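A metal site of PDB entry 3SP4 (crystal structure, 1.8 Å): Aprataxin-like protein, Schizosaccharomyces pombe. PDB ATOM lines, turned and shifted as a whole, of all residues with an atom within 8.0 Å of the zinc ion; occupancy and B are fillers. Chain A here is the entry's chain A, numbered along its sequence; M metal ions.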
ATOM      1  N   TYR A 138      15.935 -21.646 -16.901  1.00  0.00           N
ATOM      2  CA  TYR A 138      14.666 -22.347 -17.003  1.00  0.00           C
ATOM      3  C   TYR A 138      14.029 -22.560 -15.638  1.00  0.00           C
ATOM      4  O   TYR A 138      12.870 -22.215 -15.414  1.00  0.00           O
ATOM      5  CB  TYR A 138      14.868 -23.669 -17.723  1.00  0.00           C
ATOM      6  CG  TYR A 138      13.622 -24.495 -17.872  1.00  0.00           C
ATOM      7  CD1 TYR A 138      12.679 -24.198 -18.842  1.00  0.00           C
ATOM      8  CD2 TYR A 138      13.399 -25.596 -17.053  1.00  0.00           C
ATOM      9  CE1 TYR A 138      11.557 -24.960 -18.986  1.00  0.00           C
ATOM     10  CE2 TYR A 138      12.276 -26.363 -17.189  1.00  0.00           C
ATOM     11  CZ  TYR A 138      11.358 -26.050 -18.157  1.00  0.00           C
ATOM     12  OH  TYR A 138      10.246 -26.814 -18.302  1.00  0.00           O
ATOM     13  N   LYS A 171      12.495 -30.746 -16.142  1.00  0.00           N
ATOM     14  CA  LYS A 171      11.229 -31.336 -16.562  1.00  0.00           C
ATOM     15  C   LYS A 171      10.367 -30.323 -17.288  1.00  0.00           C
ATOM     16  O   LYS A 171      10.424 -29.125 -17.019  1.00  0.00           O
ATOM     17  CB  LYS A 171      10.499 -31.965 -15.383  1.00  0.00           C
ATOM     18  CG  LYS A 171      10.406 -31.125 -14.130  1.00  0.00           C
ATOM     19  CD  LYS A 171       9.327 -31.676 -13.223  1.00  0.00           C
ATOM     20  CE  LYS A 171       8.167 -32.214 -14.056  1.00  0.00           C
ATOM     21  NZ  LYS A 171       6.867 -32.381 -13.310  1.00  0.00           N
ATOM     22  N   CYS A 172       9.592 -30.803 -18.241  1.00  0.00           N
ATOM     23  CA  CYS A 172       8.757 -29.930 -19.034  1.00  0.00           C
ATOM     24  C   CYS A 172       7.646 -29.421 -18.137  1.00  0.00           C
ATOM     25  O   CYS A 172       7.034 -30.193 -17.401  1.00  0.00           O
ATOM     26  CB  CYS A 172       8.179 -30.685 -20.220  1.00  0.00           C
ATOM     27  SG  CYS A 172       7.077 -29.707 -21.273  1.00  0.00           S
ATOM     28  N   TRP A 173       7.410 -28.123 -18.204  1.00  0.00           N
ATOM     29  CA  TRP A 173       6.406 -27.487 -17.371  1.00  0.00           C
ATOM     30  C   TRP A 173       5.017 -27.881 -17.842  1.00  0.00           C
ATOM     31  O   TRP A 173       4.071 -27.924 -17.053  1.00  0.00           O
ATOM     32  CB  TRP A 173       6.577 -25.973 -17.452  1.00  0.00           C
ATOM     33  CG  TRP A 173       6.385 -25.452 -18.846  1.00  0.00           C
ATOM     34  CD1 TRP A 173       7.369 -25.187 -19.756  1.00  0.00           C
ATOM     35  CD2 TRP A 173       5.145 -25.134 -19.475  1.00  0.00           C
ATOM     36  NE1 TRP A 173       6.805 -24.730 -20.927  1.00  0.00           N
ATOM     37  CE2 TRP A 173       5.438 -24.687 -20.776  1.00  0.00           C
ATOM     38  CE3 TRP A 173       3.798 -25.182 -19.072  1.00  0.00           C
ATOM     39  CZ2 TRP A 173       4.444 -24.296 -21.672  1.00  0.00           C
ATOM     40  CZ3 TRP A 173       2.812 -24.798 -19.960  1.00  0.00           C
ATOM     41  CH2 TRP A 173       3.145 -24.359 -21.250  1.00  0.00           C
ATOM     42  N   ARG A 174       4.900 -28.187 -19.131  1.00  0.00           N
ATOM     43  CA  ARG A 174       3.597 -28.474 -19.739  1.00  0.00           C
ATOM     44  C   ARG A 174       3.158 -29.901 -19.498  1.00  0.00           C
ATOM     45  O   ARG A 174       2.000 -30.146 -19.155  1.00  0.00           O
ATOM     46  CB  ARG A 174       3.640 -28.161 -21.241  1.00  0.00           C
ATOM     47  CG  ARG A 174       2.289 -28.068 -21.921  1.00  0.00           C
ATOM     48  CD  ARG A 174       2.422 -27.309 -23.243  1.00  0.00           C
ATOM     49  NE  ARG A 174       1.131 -26.929 -23.807  1.00  0.00           N
ATOM     50  CZ  ARG A 174       0.587 -27.488 -24.874  1.00  0.00           C
ATOM     51  NH1 ARG A 174       1.224 -28.450 -25.520  1.00  0.00           N
ATOM     52  NH2 ARG A 174      -0.602 -27.074 -25.312  1.00  0.00           N
ATOM     53  N   CYS A 175       4.082 -30.847 -19.636  1.00  0.00           N
ATOM     54  CA  CYS A 175       3.716 -32.259 -19.634  1.00  0.00           C
ATOM     55  C   CYS A 175       4.476 -33.114 -18.617  1.00  0.00           C
ATOM     56  O   CYS A 175       4.159 -34.291 -18.449  1.00  0.00           O
ATOM     57  CB  CYS A 175       3.881 -32.862 -21.031  1.00  0.00           C
ATOM     58  SG  CYS A 175       5.572 -33.349 -21.430  1.00  0.00           S
ATOM     59  N   GLY A 176       5.472 -32.532 -17.964  1.00  0.00           N
ATOM     60  CA  GLY A 176       6.187 -33.231 -16.896  1.00  0.00           C
ATOM     61  C   GLY A 176       7.266 -34.231 -17.305  1.00  0.00           C
ATOM     62  O   GLY A 176       7.912 -34.838 -16.446  1.00  0.00           O
ATOM     63  N   GLU A 177       7.462 -34.430 -18.600  1.00  0.00           N
ATOM     64  CA  GLU A 177       8.552 -35.274 -19.067  1.00  0.00           C
ATOM     65  C   GLU A 177       9.885 -34.725 -18.559  1.00  0.00           C
ATOM     66  O   GLU A 177      10.106 -33.517 -18.569  1.00  0.00           O
ATOM     67  CB  GLU A 177       8.567 -35.367 -20.590  1.00  0.00           C
ATOM     68  CG  GLU A 177       9.614 -36.342 -21.139  1.00  0.00           C
ATOM     69  CD  GLU A 177       9.634 -36.419 -22.651  1.00  0.00           C
ATOM     70  OE1 GLU A 177       8.599 -36.115 -23.289  1.00  0.00           O
ATOM     71  OE2 GLU A 177      10.688 -36.769 -23.204  1.00  0.00           O
ATOM     72  N   THR A 178      10.776 -35.617 -18.120  1.00  0.00           N
ATOM     73  CA  THR A 178      12.076 -35.182 -17.589  1.00  0.00           C
ATOM     74  C   THR A 178      13.226 -35.435 -18.564  1.00  0.00           C
ATOM     75  O   THR A 178      13.152 -36.320 -19.420  1.00  0.00           O
ATOM     76  CB  THR A 178      12.399 -35.851 -16.244  1.00  0.00           C
ATOM     77  OG1 THR A 178      12.478 -37.275 -16.421  1.00  0.00           O
ATOM     78  CG2 THR A 178      11.317 -35.520 -15.216  1.00  0.00           C
ATOM     79  N   PHE A 179      14.291 -34.656 -18.417  1.00  0.00           N
ATOM     80  CA  PHE A 179      15.404 -34.688 -19.371  1.00  0.00           C
ATOM     81  C   PHE A 179      16.768 -34.701 -18.688  1.00  0.00           C
ATOM     82  O   PHE A 179      17.779 -34.372 -19.301  1.00  0.00           O
ATOM     83  CB  PHE A 179      15.319 -33.502 -20.337  1.00  0.00           C
ATOM     84  CG  PHE A 179      14.056 -33.473 -21.139  1.00  0.00           C
ATOM     85  CD1 PHE A 179      14.013 -34.028 -22.404  1.00  0.00           C
ATOM     86  CD2 PHE A 179      12.918 -32.870 -20.633  1.00  0.00           C
ATOM     87  CE1 PHE A 179      12.849 -33.995 -23.146  1.00  0.00           C
ATOM     88  CE2 PHE A 179      11.753 -32.842 -21.366  1.00  0.00           C
ATOM     89  CZ  PHE A 179      11.720 -33.400 -22.631  1.00  0.00           C
ATOM     90  N   LEU A 186      15.973 -30.698 -23.556  1.00  0.00           N
ATOM     91  CA  LEU A 186      14.848 -29.915 -23.012  1.00  0.00           C
ATOM     92  C   LEU A 186      14.452 -28.826 -23.990  1.00  0.00           C
ATOM     93  O   LEU A 186      13.272 -28.628 -24.263  1.00  0.00           O
ATOM     94  CB  LEU A 186      15.197 -29.300 -21.654  1.00  0.00           C
ATOM     95  CG  LEU A 186      14.154 -28.310 -21.131  1.00  0.00           C
ATOM     96  CD1 LEU A 186      12.831 -29.011 -20.912  1.00  0.00           C
ATOM     97  CD2 LEU A 186      14.625 -27.651 -19.850  1.00  0.00           C
ATOM     98  N   HIS A 189      12.468 -30.041 -26.982  1.00  0.00           N
ATOM     99  CA  HIS A 189      11.129 -30.415 -26.572  1.00  0.00           C
ATOM    100  C   HIS A 189      10.225 -29.209 -26.349  1.00  0.00           C
ATOM    101  O   HIS A 189       9.047 -29.229 -26.727  1.00  0.00           O
ATOM    102  CB  HIS A 189      11.191 -31.248 -25.295  1.00  0.00           C
ATOM    103  CG  HIS A 189       9.841 -31.707 -24.820  1.00  0.00           C
ATOM    104  ND1 HIS A 189       9.200 -32.807 -25.365  1.00  0.00           N
ATOM    105  CD2 HIS A 189       9.019 -31.220 -23.868  1.00  0.00           C
ATOM    106  CE1 HIS A 189       8.039 -32.973 -24.755  1.00  0.00           C
ATOM    107  NE2 HIS A 189       7.904 -32.029 -23.841  1.00  0.00           N
ATOM    108  N   LEU A 190      10.770 -28.165 -25.742  1.00  0.00           N
ATOM    109  CA  LEU A 190      10.008 -26.937 -25.514  1.00  0.00           C
ATOM    110  C   LEU A 190       9.552 -26.365 -26.849  1.00  0.00           C
ATOM    111  O   LEU A 190       8.462 -25.822 -26.979  1.00  0.00           O
ATOM    112  CB  LEU A 190      10.855 -25.892 -24.756  1.00  0.00           C
ATOM    113  CG  LEU A 190      11.156 -26.204 -23.285  1.00  0.00           C
ATOM    114  CD1 LEU A 190      12.220 -25.290 -22.766  1.00  0.00           C
ATOM    115  CD2 LEU A 190       9.871 -26.098 -22.435  1.00  0.00           C
ATOM    116  N   GLU A 192       8.873 -28.189 -29.469  1.00  0.00           N
ATOM    117  CA  GLU A 192       7.800 -29.078 -29.904  1.00  0.00           C
ATOM    118  C   GLU A 192       6.495 -28.726 -29.203  1.00  0.00           C
ATOM    119  O   GLU A 192       5.437 -28.678 -29.830  1.00  0.00           O
ATOM    120  CB  GLU A 192       8.171 -30.532 -29.622  1.00  0.00           C
ATOM    121  CG  GLU A 192       9.373 -31.033 -30.423  1.00  0.00           C
ATOM    122  CD  GLU A 192       9.712 -32.486 -30.144  1.00  0.00           C
ATOM    123  OE1 GLU A 192       8.971 -33.137 -29.375  1.00  0.00           O
ATOM    124  OE2 GLU A 192      10.728 -32.966 -30.684  1.00  0.00           O
ATOM    125  N   GLU A 193       6.583 -28.449 -27.910  1.00  0.00           N
ATOM    126  CA  GLU A 193       5.423 -28.048 -27.129  1.00  0.00           C
ATOM    127  C   GLU A 193       4.813 -26.728 -27.598  1.00  0.00           C
ATOM    128  O   GLU A 193       3.588 -26.561 -27.603  1.00  0.00           O
ATOM    129  CB  GLU A 193       5.804 -27.948 -25.651  1.00  0.00           C
ATOM    130  CG  GLU A 193       6.037 -29.277 -24.985  1.00  0.00           C
ATOM    131  CD  GLU A 193       4.742 -29.983 -24.637  1.00  0.00           C
ATOM    132  OE1 GLU A 193       3.668 -29.558 -25.115  1.00  0.00           O
ATOM    133  OE2 GLU A 193       4.800 -30.966 -23.881  1.00  0.00           O
ATOM    134  N   TYR A 194       5.666 -25.780 -27.981  1.00  0.00           N
ATOM    135  CA  TYR A 194       5.140 -24.496 -28.439  1.00  0.00           C
ATOM    136  C   TYR A 194       4.369 -24.640 -29.754  1.00  0.00           C
ATOM    137  O   TYR A 194       3.310 -24.051 -29.934  1.00  0.00           O
ATOM    138  CB  TYR A 194       6.244 -23.452 -28.598  1.00  0.00           C
ATOM    139  CG  TYR A 194       5.744 -22.211 -29.275  1.00  0.00           C
ATOM    140  CD1 TYR A 194       4.950 -21.294 -28.592  1.00  0.00           C
ATOM    141  CD2 TYR A 194       6.063 -21.952 -30.603  1.00  0.00           C
ATOM    142  CE1 TYR A 194       4.482 -20.169 -29.218  1.00  0.00           C
ATOM    143  CE2 TYR A 194       5.602 -20.805 -31.227  1.00  0.00           C
ATOM    144  CZ  TYR A 194       4.809 -19.923 -30.529  1.00  0.00           C
ATOM    145  OH  TYR A 194       4.346 -18.781 -31.145  1.00  0.00           O
HETATM  146 ZN    ZN M   1       6.301 -31.494 -22.588  1.00  0.00          ZN
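The side-chain carboxylate (OE1) of Glu 193 lies within salt-bridge range of the guanidinium group (NH1) of Arg 174. The side-chain sulfur (SG) of Cys 175 sits close to the backbone NH (N) of Glu 177, at 3.6 Å. The backbone NH (N) of Arg 174 sits close to the side-chain sulfur (SG) of Cys 172 (3.4 Å). The backbone NH (N) of Cys 172 is in hydrogen-bond range of the backbone carbonyl oxygen (O) of Glu 177 (2.8 Å).
Four residues have an atom within 4 Å of the zinc ion: Cys 172, Cys 175, His 189 and Glu 193.
The zinc ion is bound by OE2 of Glu 193 (2.1 Å). NE2 of His 189 is bound to the zinc ion (2.1 Å). The side-chain sulfur (SG) of Cys 175 binds the zinc ion, at 2.3 Å. The zinc ion is bound by SG of Cys 172 (2.4 Å).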
